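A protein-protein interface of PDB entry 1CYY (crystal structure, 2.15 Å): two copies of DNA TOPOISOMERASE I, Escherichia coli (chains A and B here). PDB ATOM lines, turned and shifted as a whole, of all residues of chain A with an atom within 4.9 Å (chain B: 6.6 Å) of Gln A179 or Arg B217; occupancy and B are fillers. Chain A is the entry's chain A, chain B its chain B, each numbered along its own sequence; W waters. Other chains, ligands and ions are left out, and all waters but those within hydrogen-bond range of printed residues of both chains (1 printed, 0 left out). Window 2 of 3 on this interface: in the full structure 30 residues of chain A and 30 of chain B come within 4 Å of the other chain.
O of Arg B217 is in hydrogen-bond range of NH2 of Arg A183. The guanidinium group of Arg B217 lies close to the side-chain amide oxygen of Gln A179 (3.5 Å).
N of Arg B217 sits at hydrogen-bond distance from O of Lys B194, 2.8 Å away. The backbone carbonyl oxygen of Asp B196 is in hydrogen-bond range of the backbone NH of Ile B215 (2.9 Å). The guanidinium group (NH1) of Arg A183 sits close to the side-chain amide nitrogen (NE2) of Gln A179, at 3.3 Å. The guanidinium group (NH1) of Arg B217 sits at hydrogen-bond distance from the backbone carbonyl oxygen (O) of Tyr B195 (3.5 Å). The guanidinium group (NH1) of Arg B217 lies within salt-bridge range of the side-chain carboxylate (OD2) of Asp B196 (2.9 Å).
Lys A176 touches Pro B62 (NZ to CG, 3.7 Å). CE of Lys A176 touches OD1 of Asp B196 (3.8 Å). CE of Lys A176 touches NH1 of Arg B217, at 3.4 Å. Pro A226 touches Leu B216. Pro A226 touches Arg B217 (CG to O, 3.7 Å).
Printed residues of chain B within 4 Å of Lys A176: Pro B62, Asp B196 and Arg B217. Trp A182 touches none of the printed residues of chain B. Printed residues of chain B within 4 Å of Arg A183: Arg B217. Of the printed residues of chain A, Pro B62 touches Lys A176 (3.7 Å). Ala B193 touches none of the printed residues of chain A. Printed residues of chain A within 4 Å of Asp B196: Lys A176 (3.8 Å). Arg B217 touches just these residues of chain A: Lys A176, Gln A179, Arg A183 and Pro A226. The nearest printed residue of chain B that does not touch Pro A226 is Phe B218 (5.0 Å).
Hydrophobic or aromatic side chains of chain B within 4 Å of the printed part of chain A: Pro B62. Hydrophobic or aromatic side chains of chain A within 4 Å of the printed part of chain B: Pro A226. Among the printed residues, no Asp or Glu carboxylate lies within 4 Å of a Lys or Arg side-chain nitrogen of the other chain.
No position is printed for both chains. Of the 7 pairs that touch across the chains among the printed residues, none has its exchanged pair printed and touching as well.
Water W1 bridges NE of Arg A183 and NZ of Lys B133.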
ATOM      1  N   ALA A 164      -4.848 -19.275  -0.591  1.00  0.00           N
ATOM      2  CA  ALA A 164      -6.242 -19.176  -0.165  1.00  0.00           C
ATOM      3  C   ALA A 164      -7.185 -19.983  -1.054  1.00  0.00           C
ATOM      4  O   ALA A 164      -8.115 -20.632  -0.572  1.00  0.00           O
ATOM      5  CB  ALA A 164      -6.670 -17.716  -0.144  1.00  0.00           C
ATOM      6  N   GLU A 165      -6.931 -19.942  -2.356  1.00  0.00           N
ATOM      7  CA  GLU A 165      -7.753 -20.655  -3.323  1.00  0.00           C
ATOM      8  C   GLU A 165      -7.826 -22.166  -3.049  1.00  0.00           C
ATOM      9  O   GLU A 165      -8.844 -22.802  -3.310  1.00  0.00           O
ATOM     10  CB  GLU A 165      -7.230 -20.380  -4.743  1.00  0.00           C
ATOM     11  CG  GLU A 165      -5.785 -19.813  -4.803  1.00  0.00           C
ATOM     12  CD  GLU A 165      -5.643 -18.371  -4.233  1.00  0.00           C
ATOM     13  OE1 GLU A 165      -4.493 -17.900  -4.071  1.00  0.00           O
ATOM     14  OE2 GLU A 165      -6.672 -17.705  -3.959  1.00  0.00           O
ATOM     15  N   GLN A 175     -11.350 -17.799   3.703  1.00  0.00           N
ATOM     16  CA  GLN A 175     -10.406 -17.806   2.594  1.00  0.00           C
ATOM     17  C   GLN A 175      -9.867 -16.403   2.373  1.00  0.00           C
ATOM     18  O   GLN A 175      -8.677 -16.224   2.168  1.00  0.00           O
ATOM     19  CB  GLN A 175     -11.078 -18.275   1.302  1.00  0.00           C
ATOM     20  CG  GLN A 175     -11.193 -19.770   1.167  1.00  0.00           C
ATOM     21  CD  GLN A 175     -11.946 -20.170  -0.098  1.00  0.00           C
ATOM     22  OE1 GLN A 175     -11.956 -19.437  -1.089  1.00  0.00           O
ATOM     23  NE2 GLN A 175     -12.567 -21.333  -0.071  1.00  0.00           N
ATOM     24  N   LYS A 176     -10.739 -15.403   2.417  1.00  0.00           N
ATOM     25  CA  LYS A 176     -10.288 -14.027   2.204  1.00  0.00           C
ATOM     26  C   LYS A 176      -9.342 -13.588   3.331  1.00  0.00           C
ATOM     27  O   LYS A 176      -8.337 -12.927   3.076  1.00  0.00           O
ATOM     28  CB  LYS A 176     -11.484 -13.067   2.122  1.00  0.00           C
ATOM     29  CG  LYS A 176     -12.120 -12.930   0.719  1.00  0.00           C
ATOM     30  CD  LYS A 176     -11.286 -12.031  -0.198  1.00  0.00           C
ATOM     31  CE  LYS A 176     -12.156 -11.226  -1.190  1.00  0.00           C
ATOM     32  NZ  LYS A 176     -12.981 -12.088  -2.142  1.00  0.00           N
ATOM     33  N   LEU A 177      -9.667 -13.963   4.566  1.00  0.00           N
ATOM     34  CA  LEU A 177      -8.827 -13.610   5.706  1.00  0.00           C
ATOM     35  C   LEU A 177      -7.488 -14.329   5.560  1.00  0.00           C
ATOM     36  O   LEU A 177      -6.429 -13.765   5.855  1.00  0.00           O
ATOM     37  CB  LEU A 177      -9.487 -14.030   7.020  1.00  0.00           C
ATOM     38  CG  LEU A 177      -8.757 -13.532   8.266  1.00  0.00           C
ATOM     39  CD1 LEU A 177      -8.838 -12.015   8.290  1.00  0.00           C
ATOM     40  CD2 LEU A 177      -9.392 -14.129   9.532  1.00  0.00           C
ATOM     41  N   TYR A 178      -7.528 -15.575   5.100  1.00  0.00           N
ATOM     42  CA  TYR A 178      -6.283 -16.320   4.914  1.00  0.00           C
ATOM     43  C   TYR A 178      -5.410 -15.634   3.861  1.00  0.00           C
ATOM     44  O   TYR A 178      -4.194 -15.515   4.024  1.00  0.00           O
ATOM     45  CB  TYR A 178      -6.559 -17.749   4.444  1.00  0.00           C
ATOM     46  CG  TYR A 178      -5.292 -18.549   4.210  1.00  0.00           C
ATOM     47  CD1 TYR A 178      -4.670 -19.220   5.257  1.00  0.00           C
ATOM     48  CD2 TYR A 178      -4.709 -18.619   2.939  1.00  0.00           C
ATOM     49  CE1 TYR A 178      -3.505 -19.946   5.053  1.00  0.00           C
ATOM     50  CE2 TYR A 178      -3.546 -19.336   2.720  1.00  0.00           C
ATOM     51  CZ  TYR A 178      -2.946 -20.007   3.785  1.00  0.00           C
ATOM     52  OH  TYR A 178      -1.824 -20.783   3.581  1.00  0.00           O
ATOM     53  N   GLN A 179      -6.024 -15.207   2.759  1.00  0.00           N
ATOM     54  CA  GLN A 179      -5.245 -14.553   1.702  1.00  0.00           C
ATOM     55  C   GLN A 179      -4.541 -13.317   2.253  1.00  0.00           C
ATOM     56  O   GLN A 179      -3.379 -13.053   1.930  1.00  0.00           O
ATOM     57  CB  GLN A 179      -6.142 -14.158   0.529  1.00  0.00           C
ATOM     58  CG  GLN A 179      -5.391 -13.452  -0.598  1.00  0.00           C
ATOM     59  CD  GLN A 179      -6.320 -13.003  -1.708  1.00  0.00           C
ATOM     60  OE1 GLN A 179      -7.278 -12.278  -1.468  1.00  0.00           O
ATOM     61  NE2 GLN A 179      -6.040 -13.439  -2.934  1.00  0.00           N
ATOM     62  N   LEU A 180      -5.254 -12.566   3.089  1.00  0.00           N
ATOM     63  CA  LEU A 180      -4.716 -11.360   3.698  1.00  0.00           C
ATOM     64  C   LEU A 180      -3.521 -11.707   4.606  1.00  0.00           C
ATOM     65  O   LEU A 180      -2.471 -11.076   4.531  1.00  0.00           O
ATOM     66  CB  LEU A 180      -5.804 -10.650   4.512  1.00  0.00           C
ATOM     67  CG  LEU A 180      -5.332  -9.385   5.241  1.00  0.00           C
ATOM     68  CD1 LEU A 180      -4.862  -8.364   4.212  1.00  0.00           C
ATOM     69  CD2 LEU A 180      -6.453  -8.815   6.103  1.00  0.00           C
ATOM     70  N   ILE A 181      -3.687 -12.716   5.451  1.00  0.00           N
ATOM     71  CA  ILE A 181      -2.606 -13.144   6.343  1.00  0.00           C
ATOM     72  C   ILE A 181      -1.419 -13.630   5.523  1.00  0.00           C
ATOM     73  O   ILE A 181      -0.279 -13.258   5.804  1.00  0.00           O
ATOM     74  CB  ILE A 181      -3.091 -14.265   7.304  1.00  0.00           C
ATOM     75  CG1 ILE A 181      -4.034 -13.659   8.348  1.00  0.00           C
ATOM     76  CG2 ILE A 181      -1.884 -14.963   7.965  1.00  0.00           C
ATOM     77  CD1 ILE A 181      -4.883 -14.679   9.102  1.00  0.00           C
ATOM     78  N   TRP A 182      -1.701 -14.438   4.497  1.00  0.00           N
ATOM     79  CA  TRP A 182      -0.676 -15.000   3.609  1.00  0.00           C
ATOM     80  C   TRP A 182       0.146 -13.902   2.923  1.00  0.00           C
ATOM     81  O   TRP A 182       1.385 -13.954   2.883  1.00  0.00           O
ATOM     82  CB  TRP A 182      -1.352 -15.893   2.540  1.00  0.00           C
ATOM     83  CG  TRP A 182      -0.403 -16.626   1.638  1.00  0.00           C
ATOM     84  CD1 TRP A 182       0.087 -17.886   1.816  1.00  0.00           C
ATOM     85  CD2 TRP A 182       0.186 -16.133   0.421  1.00  0.00           C
ATOM     86  NE1 TRP A 182       0.946 -18.212   0.785  1.00  0.00           N
ATOM     87  CE2 TRP A 182       1.025 -17.158  -0.083  1.00  0.00           C
ATOM     88  CE3 TRP A 182       0.083 -14.930  -0.292  1.00  0.00           C
ATOM     89  CZ2 TRP A 182       1.761 -17.018  -1.273  1.00  0.00           C
ATOM     90  CZ3 TRP A 182       0.819 -14.789  -1.489  1.00  0.00           C
ATOM     91  CH2 TRP A 182       1.649 -15.838  -1.958  1.00  0.00           C
ATOM     92  N   ARG A 183      -0.541 -12.893   2.399  1.00  0.00           N
ATOM     93  CA  ARG A 183       0.145 -11.796   1.704  1.00  0.00           C
ATOM     94  C   ARG A 183       1.031 -10.957   2.597  1.00  0.00           C
ATOM     95  O   ARG A 183       2.138 -10.603   2.207  1.00  0.00           O
ATOM     96  CB  ARG A 183      -0.865 -10.877   1.016  1.00  0.00           C
ATOM     97  CG  ARG A 183      -1.584 -11.530  -0.129  1.00  0.00           C
ATOM     98  CD  ARG A 183      -2.501 -10.541  -0.814  1.00  0.00           C
ATOM     99  NE  ARG A 183      -2.985 -11.073  -2.083  1.00  0.00           N
ATOM    100  CZ  ARG A 183      -3.730 -10.385  -2.942  1.00  0.00           C
ATOM    101  NH1 ARG A 183      -4.121 -10.949  -4.077  1.00  0.00           N
ATOM    102  NH2 ARG A 183      -4.084  -9.137  -2.659  1.00  0.00           N
ATOM    103  N   PRO A 226      -0.704  -5.265  -2.304  1.00  0.00           N
ATOM    104  CA  PRO A 226      -0.933  -3.919  -2.833  1.00  0.00           C
ATOM    105  C   PRO A 226      -0.900  -2.906  -1.697  1.00  0.00           C
ATOM    106  O   PRO A 226      -1.527  -3.115  -0.662  1.00  0.00           O
ATOM    107  CB  PRO A 226      -2.320  -4.032  -3.468  1.00  0.00           C
ATOM    108  CG  PRO A 226      -2.368  -5.458  -3.904  1.00  0.00           C
ATOM    109  CD  PRO A 226      -1.798  -6.169  -2.696  1.00  0.00           C
ATOM    110  N   PRO B  62     -16.754  -7.658  -2.579  1.00  0.00           N
ATOM    111  CA  PRO B  62     -15.747  -7.884  -3.622  1.00  0.00           C
ATOM    112  C   PRO B  62     -16.336  -7.536  -4.988  1.00  0.00           C
ATOM    113  O   PRO B  62     -17.476  -7.881  -5.270  1.00  0.00           O
ATOM    114  CB  PRO B  62     -15.452  -9.386  -3.513  1.00  0.00           C
ATOM    115  CG  PRO B  62     -15.858  -9.744  -2.108  1.00  0.00           C
ATOM    116  CD  PRO B  62     -17.112  -8.920  -1.911  1.00  0.00           C
ATOM    117  N   THR B  63     -15.568  -6.840  -5.821  1.00  0.00           N
ATOM    118  CA  THR B  63     -16.018  -6.486  -7.164  1.00  0.00           C
ATOM    119  C   THR B  63     -14.887  -6.774  -8.135  1.00  0.00           C
ATOM    120  O   THR B  63     -13.732  -6.910  -7.731  1.00  0.00           O
ATOM    121  CB  THR B  63     -16.413  -4.992  -7.309  1.00  0.00           C
ATOM    122  OG1 THR B  63     -15.288  -4.162  -6.990  1.00  0.00           O
ATOM    123  CG2 THR B  63     -17.593  -4.654  -6.411  1.00  0.00           C
ATOM    124  N   THR B  64     -15.223  -6.885  -9.414  1.00  0.00           N
ATOM    125  CA  THR B  64     -14.227  -7.164 -10.437  1.00  0.00           C
ATOM    126  C   THR B  64     -14.364  -6.178 -11.572  1.00  0.00           C
ATOM    127  O   THR B  64     -15.429  -5.593 -11.788  1.00  0.00           O
ATOM    128  CB  THR B  64     -14.394  -8.561 -11.043  1.00  0.00           C
ATOM    129  OG1 THR B  64     -15.665  -8.637 -11.700  1.00  0.00           O
ATOM    130  CG2 THR B  64     -14.319  -9.631  -9.968  1.00  0.00           C
ATOM    131  N   LYS B 133      -1.638 -16.140 -12.053  1.00  0.00           N
ATOM    132  CA  LYS B 133      -2.872 -15.453 -11.716  1.00  0.00           C
ATOM    133  C   LYS B 133      -3.334 -14.516 -12.828  1.00  0.00           C
ATOM    134  O   LYS B 133      -4.472 -14.072 -12.824  1.00  0.00           O
ATOM    135  CB  LYS B 133      -2.703 -14.706 -10.387  1.00  0.00           C
ATOM    136  CG  LYS B 133      -2.700 -15.664  -9.187  1.00  0.00           C
ATOM    137  CD  LYS B 133      -2.435 -14.996  -7.836  1.00  0.00           C
ATOM    138  CE  LYS B 133      -0.954 -14.677  -7.613  1.00  0.00           C
ATOM    139  NZ  LYS B 133      -0.596 -14.647  -6.148  1.00  0.00           N
ATOM    140  N   ALA B 193      -9.333  -7.498 -12.920  1.00  0.00           N
ATOM    141  CA  ALA B 193      -8.678  -6.844 -11.789  1.00  0.00           C
ATOM    142  C   ALA B 193      -9.723  -7.036 -10.696  1.00  0.00           C
ATOM    143  O   ALA B 193     -10.913  -7.062 -10.997  1.00  0.00           O
ATOM    144  CB  ALA B 193      -8.465  -5.371 -12.072  1.00  0.00           C
ATOM    145  N   LYS B 194      -9.299  -7.207  -9.447  1.00  0.00           N
ATOM    146  CA  LYS B 194     -10.258  -7.412  -8.367  1.00  0.00           C
ATOM    147  C   LYS B 194     -10.096  -6.368  -7.281  1.00  0.00           C
ATOM    148  O   LYS B 194      -8.984  -5.921  -6.992  1.00  0.00           O
ATOM    149  CB  LYS B 194     -10.106  -8.817  -7.760  1.00  0.00           C
ATOM    150  CG  LYS B 194      -9.999  -9.932  -8.820  1.00  0.00           C
ATOM    151  CD  LYS B 194     -10.404 -11.306  -8.283  1.00  0.00           C
ATOM    152  CE  LYS B 194     -11.928 -11.497  -8.332  1.00  0.00           C
ATOM    153  NZ  LYS B 194     -12.404 -12.824  -7.775  1.00  0.00           N
ATOM    154  N   TYR B 195     -11.218  -5.984  -6.683  1.00  0.00           N
ATOM    155  CA  TYR B 195     -11.215  -4.984  -5.627  1.00  0.00           C
ATOM    156  C   TYR B 195     -12.168  -5.340  -4.502  1.00  0.00           C
ATOM    157  O   TYR B 195     -13.025  -6.214  -4.632  1.00  0.00           O
ATOM    158  CB  TYR B 195     -11.677  -3.620  -6.152  1.00  0.00           C
ATOM    159  CG  TYR B 195     -10.972  -3.112  -7.382  1.00  0.00           C
ATOM    160  CD1 TYR B 195     -11.294  -3.598  -8.647  1.00  0.00           C
ATOM    161  CD2 TYR B 195      -9.997  -2.117  -7.284  1.00  0.00           C
ATOM    162  CE1 TYR B 195     -10.661  -3.098  -9.797  1.00  0.00           C
ATOM    163  CE2 TYR B 195      -9.357  -1.613  -8.425  1.00  0.00           C
ATOM    164  CZ  TYR B 195      -9.696  -2.112  -9.674  1.00  0.00           C
ATOM    165  OH  TYR B 195      -9.044  -1.651 -10.784  1.00  0.00           O
ATOM    166  N   ASP B 196     -12.014  -4.622  -3.398  1.00  0.00           N
ATOM    167  CA  ASP B 196     -12.899  -4.764  -2.264  1.00  0.00           C
ATOM    168  C   ASP B 196     -13.505  -3.365  -2.160  1.00  0.00           C
ATOM    169  O   ASP B 196     -12.816  -2.400  -1.818  1.00  0.00           O
ATOM    170  CB  ASP B 196     -12.107  -5.177  -1.031  1.00  0.00           C
ATOM    171  CG  ASP B 196     -11.824  -6.677  -1.022  1.00  0.00           C
ATOM    172  OD1 ASP B 196     -12.799  -7.449  -0.892  1.00  0.00           O
ATOM    173  OD2 ASP B 196     -10.655  -7.089  -1.164  1.00  0.00           O
ATOM    174  N   ILE B 215     -10.592  -0.800  -2.694  1.00  0.00           N
ATOM    175  CA  ILE B 215      -9.218  -1.186  -2.449  1.00  0.00           C
ATOM    176  C   ILE B 215      -8.804  -2.233  -3.480  1.00  0.00           C
ATOM    177  O   ILE B 215      -9.459  -3.274  -3.623  1.00  0.00           O
ATOM    178  CB  ILE B 215      -9.100  -1.788  -1.031  1.00  0.00           C
ATOM    179  CG1 ILE B 215      -9.391  -0.702   0.007  1.00  0.00           C
ATOM    180  CG2 ILE B 215      -7.738  -2.421  -0.831  1.00  0.00           C
ATOM    181  CD1 ILE B 215      -9.514  -1.226   1.435  1.00  0.00           C
ATOM    182  N   LEU B 216      -7.714  -1.957  -4.188  1.00  0.00           N
ATOM    183  CA  LEU B 216      -7.200  -2.884  -5.187  1.00  0.00           C
ATOM    184  C   LEU B 216      -6.639  -4.143  -4.528  1.00  0.00           C
ATOM    185  O   LEU B 216      -5.777  -4.055  -3.639  1.00  0.00           O
ATOM    186  CB  LEU B 216      -6.087  -2.221  -5.990  1.00  0.00           C
ATOM    187  CG  LEU B 216      -5.245  -3.136  -6.877  1.00  0.00           C
ATOM    188  CD1 LEU B 216      -6.081  -3.622  -8.054  1.00  0.00           C
ATOM    189  CD2 LEU B 216      -4.019  -2.380  -7.367  1.00  0.00           C
ATOM    190  N   ARG B 217      -7.129  -5.305  -4.953  1.00  0.00           N
ATOM    191  CA  ARG B 217      -6.641  -6.569  -4.428  1.00  0.00           C
ATOM    192  C   ARG B 217      -5.782  -7.300  -5.478  1.00  0.00           C
ATOM    193  O   ARG B 217      -4.825  -7.980  -5.140  1.00  0.00           O
ATOM    194  CB  ARG B 217      -7.805  -7.456  -3.974  1.00  0.00           C
ATOM    195  CG  ARG B 217      -7.356  -8.552  -3.008  1.00  0.00           C
ATOM    196  CD  ARG B 217      -8.513  -9.365  -2.411  1.00  0.00           C
ATOM    197  NE  ARG B 217      -9.227 -10.145  -3.424  1.00  0.00           N
ATOM    198  CZ  ARG B 217     -10.447  -9.859  -3.871  1.00  0.00           C
ATOM    199  NH1 ARG B 217     -11.109  -8.810  -3.398  1.00  0.00           N
ATOM    200  NH2 ARG B 217     -11.005 -10.623  -4.800  1.00  0.00           N
ATOM    201  N   PHE B 218      -6.115  -7.142  -6.754  1.00  0.00           N
ATOM    202  CA  PHE B 218      -5.352  -7.780  -7.828  1.00  0.00           C
ATOM    203  C   PHE B 218      -5.469  -6.916  -9.084  1.00  0.00           C
ATOM    204  O   PHE B 218      -6.578  -6.641  -9.548  1.00  0.00           O
ATOM    205  CB  PHE B 218      -5.892  -9.186  -8.086  1.00  0.00           C
ATOM    206  CG  PHE B 218      -5.176  -9.910  -9.174  1.00  0.00           C
ATOM    207  CD1 PHE B 218      -3.802 -10.106  -9.102  1.00  0.00           C
ATOM    208  CD2 PHE B 218      -5.862 -10.344 -10.308  1.00  0.00           C
ATOM    209  CE1 PHE B 218      -3.115 -10.717 -10.150  1.00  0.00           C
ATOM    210  CE2 PHE B 218      -5.187 -10.960 -11.364  1.00  0.00           C
ATOM    211  CZ  PHE B 218      -3.815 -11.145 -11.289  1.00  0.00           C
ATOM    212  N   ASP B 219      -4.338  -6.486  -9.637  1.00  0.00           N
ATOM    213  CA  ASP B 219      -4.382  -5.613 -10.808  1.00  0.00           C
ATOM    214  C   ASP B 219      -4.778  -6.290 -12.123  1.00  0.00           C
ATOM    215  O   ASP B 219      -5.373  -5.648 -12.994  1.00  0.00           O
ATOM    216  CB  ASP B 219      -3.054  -4.837 -10.965  1.00  0.00           C
ATOM    217  CG  ASP B 219      -1.825  -5.743 -11.102  1.00  0.00           C
ATOM    218  OD1 ASP B 219      -1.925  -6.977 -10.931  1.00  0.00           O
ATOM    219  OD2 ASP B 219      -0.730  -5.193 -11.374  1.00  0.00           O
HETATM  220  O   HOH W   1      -2.329 -13.634  -3.603  1.00  0.00           O
